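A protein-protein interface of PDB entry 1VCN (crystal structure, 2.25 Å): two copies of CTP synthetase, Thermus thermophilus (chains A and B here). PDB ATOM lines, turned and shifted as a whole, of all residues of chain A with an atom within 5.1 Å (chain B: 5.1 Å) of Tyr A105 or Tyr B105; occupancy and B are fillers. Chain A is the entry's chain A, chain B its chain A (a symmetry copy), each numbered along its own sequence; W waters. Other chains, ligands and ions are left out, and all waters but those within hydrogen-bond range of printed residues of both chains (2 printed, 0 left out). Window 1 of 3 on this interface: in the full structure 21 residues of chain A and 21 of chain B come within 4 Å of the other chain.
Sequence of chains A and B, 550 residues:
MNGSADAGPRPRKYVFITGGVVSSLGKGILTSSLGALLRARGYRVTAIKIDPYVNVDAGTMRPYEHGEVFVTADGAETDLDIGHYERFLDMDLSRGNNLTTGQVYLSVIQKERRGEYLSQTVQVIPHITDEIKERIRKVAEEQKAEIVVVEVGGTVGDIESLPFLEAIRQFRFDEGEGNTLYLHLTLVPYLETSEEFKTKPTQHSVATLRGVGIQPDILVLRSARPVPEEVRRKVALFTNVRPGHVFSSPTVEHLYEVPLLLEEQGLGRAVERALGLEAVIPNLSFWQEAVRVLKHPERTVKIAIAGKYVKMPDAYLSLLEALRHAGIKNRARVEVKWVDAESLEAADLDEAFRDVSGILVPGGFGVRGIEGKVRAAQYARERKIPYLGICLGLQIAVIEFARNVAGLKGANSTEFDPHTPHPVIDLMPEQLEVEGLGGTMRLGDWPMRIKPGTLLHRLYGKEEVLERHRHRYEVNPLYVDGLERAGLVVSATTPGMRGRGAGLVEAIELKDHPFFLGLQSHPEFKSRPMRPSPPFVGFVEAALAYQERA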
ATOM      1  N   VAL A  54      10.594  13.564 -35.268  1.00  0.00           N
ATOM      2  CA  VAL A  54      11.749  14.267 -34.734  1.00  0.00           C
ATOM      3  C   VAL A  54      11.909  15.714 -35.236  1.00  0.00           C
ATOM      4  O   VAL A  54      12.681  16.486 -34.667  1.00  0.00           O
ATOM      5  CB  VAL A  54      13.040  13.472 -35.023  1.00  0.00           C
ATOM      6  CG1 VAL A  54      14.241  14.200 -34.447  1.00  0.00           C
ATOM      7  CG2 VAL A  54      12.939  12.055 -34.414  1.00  0.00           C
ATOM      8  N   THR A 101       8.585  15.612 -31.042  1.00  0.00           N
ATOM      9  CA  THR A 101       9.665  14.927 -30.355  1.00  0.00           C
ATOM     10  C   THR A 101      10.930  15.793 -30.387  1.00  0.00           C
ATOM     11  O   THR A 101      11.660  15.862 -29.402  1.00  0.00           O
ATOM     12  CB  THR A 101       9.960  13.566 -31.021  1.00  0.00           C
ATOM     13  OG1 THR A 101       8.842  12.693 -30.838  1.00  0.00           O
ATOM     14  CG2 THR A 101      11.207  12.924 -30.415  1.00  0.00           C
ATOM     15  N   GLY A 102      11.180  16.459 -31.517  1.00  0.00           N
ATOM     16  CA  GLY A 102      12.370  17.296 -31.653  1.00  0.00           C
ATOM     17  C   GLY A 102      12.418  18.457 -30.671  1.00  0.00           C
ATOM     18  O   GLY A 102      13.441  18.715 -30.034  1.00  0.00           O
ATOM     19  N   GLN A 103      11.303  19.170 -30.576  1.00  0.00           N
ATOM     20  CA  GLN A 103      11.159  20.289 -29.653  1.00  0.00           C
ATOM     21  C   GLN A 103      11.483  19.820 -28.240  1.00  0.00           C
ATOM     22  O   GLN A 103      12.324  20.384 -27.549  1.00  0.00           O
ATOM     23  CB  GLN A 103       9.708  20.791 -29.664  1.00  0.00           C
ATOM     24  CG  GLN A 103       9.335  21.704 -30.815  1.00  0.00           C
ATOM     25  CD  GLN A 103       7.832  21.928 -30.924  1.00  0.00           C
ATOM     26  OE1 GLN A 103       7.103  21.837 -29.941  1.00  0.00           O
ATOM     27  NE2 GLN A 103       7.368  22.231 -32.127  1.00  0.00           N
ATOM     28  N   VAL A 104      10.797  18.769 -27.821  1.00  0.00           N
ATOM     29  CA  VAL A 104      10.959  18.245 -26.481  1.00  0.00           C
ATOM     30  C   VAL A 104      12.377  17.816 -26.165  1.00  0.00           C
ATOM     31  O   VAL A 104      12.931  18.199 -25.133  1.00  0.00           O
ATOM     32  CB  VAL A 104       9.977  17.083 -26.240  1.00  0.00           C
ATOM     33  CG1 VAL A 104      10.325  16.357 -24.973  1.00  0.00           C
ATOM     34  CG2 VAL A 104       8.557  17.634 -26.144  1.00  0.00           C
ATOM     35  N   TYR A 105      12.978  17.030 -27.046  1.00  0.00           N
ATOM     36  CA  TYR A 105      14.328  16.579 -26.799  1.00  0.00           C
ATOM     37  C   TYR A 105      15.339  17.711 -26.887  1.00  0.00           C
ATOM     38  O   TYR A 105      16.241  17.793 -26.064  1.00  0.00           O
ATOM     39  CB  TYR A 105      14.714  15.457 -27.772  1.00  0.00           C
ATOM     40  CG  TYR A 105      14.277  14.068 -27.320  1.00  0.00           C
ATOM     41  CD1 TYR A 105      12.939  13.676 -27.390  1.00  0.00           C
ATOM     42  CD2 TYR A 105      15.215  13.134 -26.862  1.00  0.00           C
ATOM     43  CE1 TYR A 105      12.545  12.391 -27.024  1.00  0.00           C
ATOM     44  CE2 TYR A 105      14.826  11.842 -26.491  1.00  0.00           C
ATOM     45  CZ  TYR A 105      13.489  11.477 -26.576  1.00  0.00           C
ATOM     46  OH  TYR A 105      13.095  10.200 -26.214  1.00  0.00           O
ATOM     47  N   LEU A 106      15.194  18.573 -27.887  1.00  0.00           N
ATOM     48  CA  LEU A 106      16.117  19.686 -28.065  1.00  0.00           C
ATOM     49  C   LEU A 106      16.092  20.588 -26.834  1.00  0.00           C
ATOM     50  O   LEU A 106      17.135  21.032 -26.326  1.00  0.00           O
ATOM     51  CB  LEU A 106      15.728  20.493 -29.311  1.00  0.00           C
ATOM     52  CG  LEU A 106      16.527  21.768 -29.590  1.00  0.00           C
ATOM     53  CD1 LEU A 106      18.015  21.442 -29.667  1.00  0.00           C
ATOM     54  CD2 LEU A 106      16.051  22.396 -30.896  1.00  0.00           C
ATOM     55  N   SER A 107      14.879  20.847 -26.366  1.00  0.00           N
ATOM     56  CA  SER A 107      14.644  21.680 -25.200  1.00  0.00           C
ATOM     57  C   SER A 107      15.350  21.102 -23.966  1.00  0.00           C
ATOM     58  O   SER A 107      16.140  21.779 -23.300  1.00  0.00           O
ATOM     59  CB  SER A 107      13.129  21.776 -24.978  1.00  0.00           C
ATOM     60  OG  SER A 107      12.806  22.397 -23.757  1.00  0.00           O
ATOM     61  N   VAL A 108      15.083  19.840 -23.673  1.00  0.00           N
ATOM     62  CA  VAL A 108      15.695  19.210 -22.518  1.00  0.00           C
ATOM     63  C   VAL A 108      17.208  19.100 -22.656  1.00  0.00           C
ATOM     64  O   VAL A 108      17.936  19.282 -21.683  1.00  0.00           O
ATOM     65  CB  VAL A 108      15.083  17.821 -22.283  1.00  0.00           C
ATOM     66  CG1 VAL A 108      15.856  17.067 -21.198  1.00  0.00           C
ATOM     67  CG2 VAL A 108      13.631  17.985 -21.876  1.00  0.00           C
ATOM     68  N   ILE A 109      17.680  18.811 -23.864  1.00  0.00           N
ATOM     69  CA  ILE A 109      19.111  18.683 -24.091  1.00  0.00           C
ATOM     70  C   ILE A 109      19.837  20.002 -23.830  1.00  0.00           C
ATOM     71  O   ILE A 109      20.860  20.034 -23.139  1.00  0.00           O
ATOM     72  CB  ILE A 109      19.411  18.199 -25.541  1.00  0.00           C
ATOM     73  CG1 ILE A 109      19.041  16.717 -25.682  1.00  0.00           C
ATOM     74  CG2 ILE A 109      20.901  18.382 -25.864  1.00  0.00           C
ATOM     75  CD1 ILE A 109      19.197  16.164 -27.095  1.00  0.00           C
ATOM     76  N   GLN A 110      19.309  21.092 -24.378  1.00  0.00           N
ATOM     77  CA  GLN A 110      19.934  22.397 -24.187  1.00  0.00           C
ATOM     78  C   GLN A 110      19.946  22.791 -22.711  1.00  0.00           C
ATOM     79  O   GLN A 110      20.865  23.463 -22.257  1.00  0.00           O
ATOM     80  CB  GLN A 110      19.220  23.458 -25.025  1.00  0.00           C
ATOM     81  CG  GLN A 110      19.281  23.185 -26.517  1.00  0.00           C
ATOM     82  CD  GLN A 110      18.516  24.206 -27.328  1.00  0.00           C
ATOM     83  OE1 GLN A 110      17.389  24.559 -26.996  1.00  0.00           O
ATOM     84  NE2 GLN A 110      19.125  24.681 -28.405  1.00  0.00           N
ATOM     85  N   VAL A 124      14.761   9.795 -20.128  1.00  0.00           N
ATOM     86  CA  VAL A 124      13.485   9.976 -20.813  1.00  0.00           C
ATOM     87  C   VAL A 124      12.416  10.181 -19.746  1.00  0.00           C
ATOM     88  O   VAL A 124      11.597  11.097 -19.831  1.00  0.00           O
ATOM     89  CB  VAL A 124      13.166   8.741 -21.695  1.00  0.00           C
ATOM     90  CG1 VAL A 124      11.773   8.842 -22.291  1.00  0.00           C
ATOM     91  CG2 VAL A 124      14.193   8.658 -22.813  1.00  0.00           C
ATOM     92  N   ILE A 128      12.230  13.943 -19.920  1.00  0.00           N
ATOM     93  CA  ILE A 128      11.551  14.201 -21.184  1.00  0.00           C
ATOM     94  C   ILE A 128      10.056  14.267 -20.921  1.00  0.00           C
ATOM     95  O   ILE A 128       9.358  15.124 -21.461  1.00  0.00           O
ATOM     96  CB  ILE A 128      11.797  13.091 -22.233  1.00  0.00           C
ATOM     97  CG1 ILE A 128      13.286  12.988 -22.590  1.00  0.00           C
ATOM     98  CG2 ILE A 128      10.993  13.402 -23.486  1.00  0.00           C
ATOM     99  CD1 ILE A 128      13.814  14.160 -23.403  1.00  0.00           C
ATOM    100  N   PRO A 163       7.228   8.195 -25.188  1.00  0.00           N
ATOM    101  CA  PRO A 163       7.424   9.267 -24.201  1.00  0.00           C
ATOM    102  C   PRO A 163       6.155  10.098 -24.013  1.00  0.00           C
ATOM    103  O   PRO A 163       5.870  10.573 -22.914  1.00  0.00           O
ATOM    104  CB  PRO A 163       8.567  10.089 -24.798  1.00  0.00           C
ATOM    105  CG  PRO A 163       9.326   9.071 -25.614  1.00  0.00           C
ATOM    106  CD  PRO A 163       8.203   8.308 -26.278  1.00  0.00           C
ATOM    107  N   VAL B  54      20.018  11.071 -21.648  1.00  0.00           N
ATOM    108  CA  VAL B  54      19.881  12.203 -22.549  1.00  0.00           C
ATOM    109  C   VAL B  54      21.067  13.185 -22.535  1.00  0.00           C
ATOM    110  O   VAL B  54      21.188  14.025 -23.426  1.00  0.00           O
ATOM    111  CB  VAL B  54      18.572  12.966 -22.254  1.00  0.00           C
ATOM    112  CG1 VAL B  54      18.422  14.135 -23.211  1.00  0.00           C
ATOM    113  CG2 VAL B  54      17.361  12.015 -22.388  1.00  0.00           C
ATOM    114  N   THR B 101      22.101   9.153 -25.900  1.00  0.00           N
ATOM    115  CA  THR B 101      20.836   9.505 -26.520  1.00  0.00           C
ATOM    116  C   THR B 101      20.865  10.975 -26.956  1.00  0.00           C
ATOM    117  O   THR B 101      20.362  11.316 -28.024  1.00  0.00           O
ATOM    118  CB  THR B 101      19.665   9.287 -25.537  1.00  0.00           C
ATOM    119  OG1 THR B 101      19.525   7.889 -25.266  1.00  0.00           O
ATOM    120  CG2 THR B 101      18.359   9.822 -26.122  1.00  0.00           C
ATOM    121  N   GLY B 102      21.463  11.840 -26.133  1.00  0.00           N
ATOM    122  CA  GLY B 102      21.527  13.264 -26.451  1.00  0.00           C
ATOM    123  C   GLY B 102      22.293  13.574 -27.727  1.00  0.00           C
ATOM    124  O   GLY B 102      21.844  14.351 -28.572  1.00  0.00           O
ATOM    125  N   GLN B 103      23.471  12.974 -27.844  1.00  0.00           N
ATOM    126  CA  GLN B 103      24.318  13.123 -29.021  1.00  0.00           C
ATOM    127  C   GLN B 103      23.523  12.742 -30.265  1.00  0.00           C
ATOM    128  O   GLN B 103      23.415  13.502 -31.220  1.00  0.00           O
ATOM    129  CB  GLN B 103      25.522  12.177 -28.921  1.00  0.00           C
ATOM    130  CG  GLN B 103      26.666  12.654 -28.049  1.00  0.00           C
ATOM    131  CD  GLN B 103      27.686  11.559 -27.766  1.00  0.00           C
ATOM    132  OE1 GLN B 103      27.846  10.622 -28.543  1.00  0.00           O
ATOM    133  NE2 GLN B 103      28.386  11.682 -26.648  1.00  0.00           N
ATOM    134  N   VAL B 104      22.962  11.544 -30.232  1.00  0.00           N
ATOM    135  CA  VAL B 104      22.222  11.025 -31.364  1.00  0.00           C
ATOM    136  C   VAL B 104      21.046  11.890 -31.767  1.00  0.00           C
ATOM    137  O   VAL B 104      20.889  12.224 -32.942  1.00  0.00           O
ATOM    138  CB  VAL B 104      21.761   9.582 -31.083  1.00  0.00           C
ATOM    139  CG1 VAL B 104      20.765   9.140 -32.116  1.00  0.00           C
ATOM    140  CG2 VAL B 104      22.972   8.653 -31.103  1.00  0.00           C
ATOM    141  N   TYR B 105      20.218  12.265 -30.804  1.00  0.00           N
ATOM    142  CA  TYR B 105      19.071  13.084 -31.124  1.00  0.00           C
ATOM    143  C   TYR B 105      19.466  14.490 -31.545  1.00  0.00           C
ATOM    144  O   TYR B 105      18.907  15.027 -32.492  1.00  0.00           O
ATOM    145  CB  TYR B 105      18.098  13.147 -29.939  1.00  0.00           C
ATOM    146  CG  TYR B 105      17.119  11.980 -29.879  1.00  0.00           C
ATOM    147  CD1 TYR B 105      17.536  10.711 -29.476  1.00  0.00           C
ATOM    148  CD2 TYR B 105      15.764  12.163 -30.186  1.00  0.00           C
ATOM    149  CE1 TYR B 105      16.633   9.654 -29.373  1.00  0.00           C
ATOM    150  CE2 TYR B 105      14.852  11.106 -30.086  1.00  0.00           C
ATOM    151  CZ  TYR B 105      15.294   9.855 -29.677  1.00  0.00           C
ATOM    152  OH  TYR B 105      14.398   8.805 -29.573  1.00  0.00           O
ATOM    153  N   LEU B 106      20.420  15.086 -30.837  1.00  0.00           N
ATOM    154  CA  LEU B 106      20.862  16.437 -31.153  1.00  0.00           C
ATOM    155  C   LEU B 106      21.415  16.488 -32.575  1.00  0.00           C
ATOM    156  O   LEU B 106      21.129  17.410 -33.357  1.00  0.00           O
ATOM    157  CB  LEU B 106      21.943  16.879 -30.157  1.00  0.00           C
ATOM    158  CG  LEU B 106      22.604  18.237 -30.406  1.00  0.00           C
ATOM    159  CD1 LEU B 106      21.538  19.326 -30.482  1.00  0.00           C
ATOM    160  CD2 LEU B 106      23.594  18.538 -29.286  1.00  0.00           C
ATOM    161  N   SER B 107      22.211  15.476 -32.892  1.00  0.00           N
ATOM    162  CA  SER B 107      22.831  15.339 -34.197  1.00  0.00           C
ATOM    163  C   SER B 107      21.769  15.274 -35.302  1.00  0.00           C
ATOM    164  O   SER B 107      21.786  16.053 -36.260  1.00  0.00           O
ATOM    165  CB  SER B 107      23.699  14.074 -34.185  1.00  0.00           C
ATOM    166  OG  SER B 107      24.184  13.745 -35.465  1.00  0.00           O
ATOM    167  N   VAL B 108      20.828  14.355 -35.158  1.00  0.00           N
ATOM    168  CA  VAL B 108      19.786  14.209 -36.158  1.00  0.00           C
ATOM    169  C   VAL B 108      18.895  15.441 -36.245  1.00  0.00           C
ATOM    170  O   VAL B 108      18.488  15.840 -37.334  1.00  0.00           O
ATOM    171  CB  VAL B 108      18.937  12.963 -35.865  1.00  0.00           C
ATOM    172  CG1 VAL B 108      17.718  12.911 -36.789  1.00  0.00           C
ATOM    173  CG2 VAL B 108      19.795  11.728 -36.057  1.00  0.00           C
ATOM    174  N   ILE B 109      18.599  16.049 -35.101  1.00  0.00           N
ATOM    175  CA  ILE B 109      17.753  17.233 -35.085  1.00  0.00           C
ATOM    176  C   ILE B 109      18.400  18.391 -35.842  1.00  0.00           C
ATOM    177  O   ILE B 109      17.756  19.042 -36.670  1.00  0.00           O
ATOM    178  CB  ILE B 109      17.430  17.676 -33.628  1.00  0.00           C
ATOM    179  CG1 ILE B 109      16.436  16.695 -32.993  1.00  0.00           C
ATOM    180  CG2 ILE B 109      16.824  19.086 -33.624  1.00  0.00           C
ATOM    181  CD1 ILE B 109      16.129  16.976 -31.525  1.00  0.00           C
ATOM    182  N   GLN B 110      19.674  18.648 -35.564  1.00  0.00           N
ATOM    183  CA  GLN B 110      20.376  19.738 -36.236  1.00  0.00           C
ATOM    184  C   GLN B 110      20.450  19.499 -37.742  1.00  0.00           C
ATOM    185  O   GLN B 110      20.428  20.445 -38.522  1.00  0.00           O
ATOM    186  CB  GLN B 110      21.776  19.914 -35.646  1.00  0.00           C
ATOM    187  CG  GLN B 110      21.763  20.275 -34.171  1.00  0.00           C
ATOM    188  CD  GLN B 110      23.153  20.382 -33.586  1.00  0.00           C
ATOM    189  OE1 GLN B 110      24.002  19.527 -33.817  1.00  0.00           O
ATOM    190  NE2 GLN B 110      23.391  21.434 -32.816  1.00  0.00           N
ATOM    191  N   VAL B 124      12.155   8.168 -35.450  1.00  0.00           N
ATOM    192  CA  VAL B 124      13.111   7.410 -34.650  1.00  0.00           C
ATOM    193  C   VAL B 124      13.685   6.313 -35.538  1.00  0.00           C
ATOM    194  O   VAL B 124      14.899   6.108 -35.595  1.00  0.00           O
ATOM    195  CB  VAL B 124      12.414   6.812 -33.401  1.00  0.00           C
ATOM    196  CG1 VAL B 124      13.354   5.892 -32.641  1.00  0.00           C
ATOM    197  CG2 VAL B 124      11.971   7.949 -32.494  1.00  0.00           C
ATOM    198  N   ILE B 128      16.910   8.035 -36.463  1.00  0.00           N
ATOM    199  CA  ILE B 128      17.700   7.977 -35.239  1.00  0.00           C
ATOM    200  C   ILE B 128      18.524   6.700 -35.260  1.00  0.00           C
ATOM    201  O   ILE B 128      19.698   6.702 -34.892  1.00  0.00           O
ATOM    202  CB  ILE B 128      16.826   7.953 -33.963  1.00  0.00           C
ATOM    203  CG1 ILE B 128      15.991   9.234 -33.843  1.00  0.00           C
ATOM    204  CG2 ILE B 128      17.726   7.816 -32.744  1.00  0.00           C
ATOM    205  CD1 ILE B 128      16.801  10.479 -33.514  1.00  0.00           C
ATOM    206  N   PRO B 163      15.772   2.702 -28.974  1.00  0.00           N
ATOM    207  CA  PRO B 163      16.385   3.089 -30.254  1.00  0.00           C
ATOM    208  C   PRO B 163      17.727   2.391 -30.469  1.00  0.00           C
ATOM    209  O   PRO B 163      18.092   2.060 -31.596  1.00  0.00           O
ATOM    210  CB  PRO B 163      16.537   4.604 -30.125  1.00  0.00           C
ATOM    211  CG  PRO B 163      15.421   4.979 -29.180  1.00  0.00           C
ATOM    212  CD  PRO B 163      15.514   3.883 -28.143  1.00  0.00           C
HETATM  213  O   HOH W   1      11.921   9.211 -28.853  1.00  0.00           O
HETATM  214  O   HOH W   2      14.659   8.145 -26.604  1.00  0.00           O
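O of Val A54 lies close to N of Gly A102. The backbone NH of Gly B102 sits close to the backbone carbonyl oxygen of Val B54 (3.5 Å).
Val A54 touches Ile B109. CD1 of Ile B109 touches O of Gly A102, 3.5 Å away. CD2 of Tyr B105 touches CD2 of Tyr A105, at 3.5 Å. Ile A109 touches Val B54. CD1 of Ile A109 touches O of Gly B102 (3.5 Å).
Tyr A105 touches just one residue of chain B: Tyr B105 (3.5 Å). Tyr B105 touches just one residue of chain A: Tyr A105. Of the printed residues of chain B, Ile A109 touches Val B54 (3.6 Å) and Gly B102 (3.5 Å). Printed residues of chain A within 4 Å of Val B54: Ile A109. Of the printed residues of chain B, Val A54 touches Ile B109. Of the printed residues of chain A, Gly B102 touches Ile A109. Printed residues of chain A within 4 Å of Ile B109: Val A54 (3.6 Å) and Gly A102 (3.5 Å). The nearest residue of chain B that does not touch Tyr A105 is Thr B101 (4.1 Å). The nearest residue of chain A that does not touch Tyr B105 is Thr A101 (4.1 Å). The nearest printed residue of chain A that does not touch Gly B102 is Tyr A105 (6.3 Å).
Among the printed residues, no Asp or Glu carboxylate lies within 4 Å of a Lys or Arg side-chain nitrogen of the other chain.
Val A54 touches Ile B109, and with the chains exchanged Ile A109 touches Val B54. Gly A102 touches Ile B109, and with the chains exchanged Ile A109 touches Gly B102. Tyr A105 touches its own counterpart, Tyr B105. Of the 5 pairs that touch across the chains among the printed residues, 5 have their exchanged pair printed and touching as well.
Water W2 bridges OH of Tyr A105 (2.6 Å) and OH of Tyr B105 (3.1 Å). Water W1 bridges OH of Tyr B105 and OH of Tyr A105.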
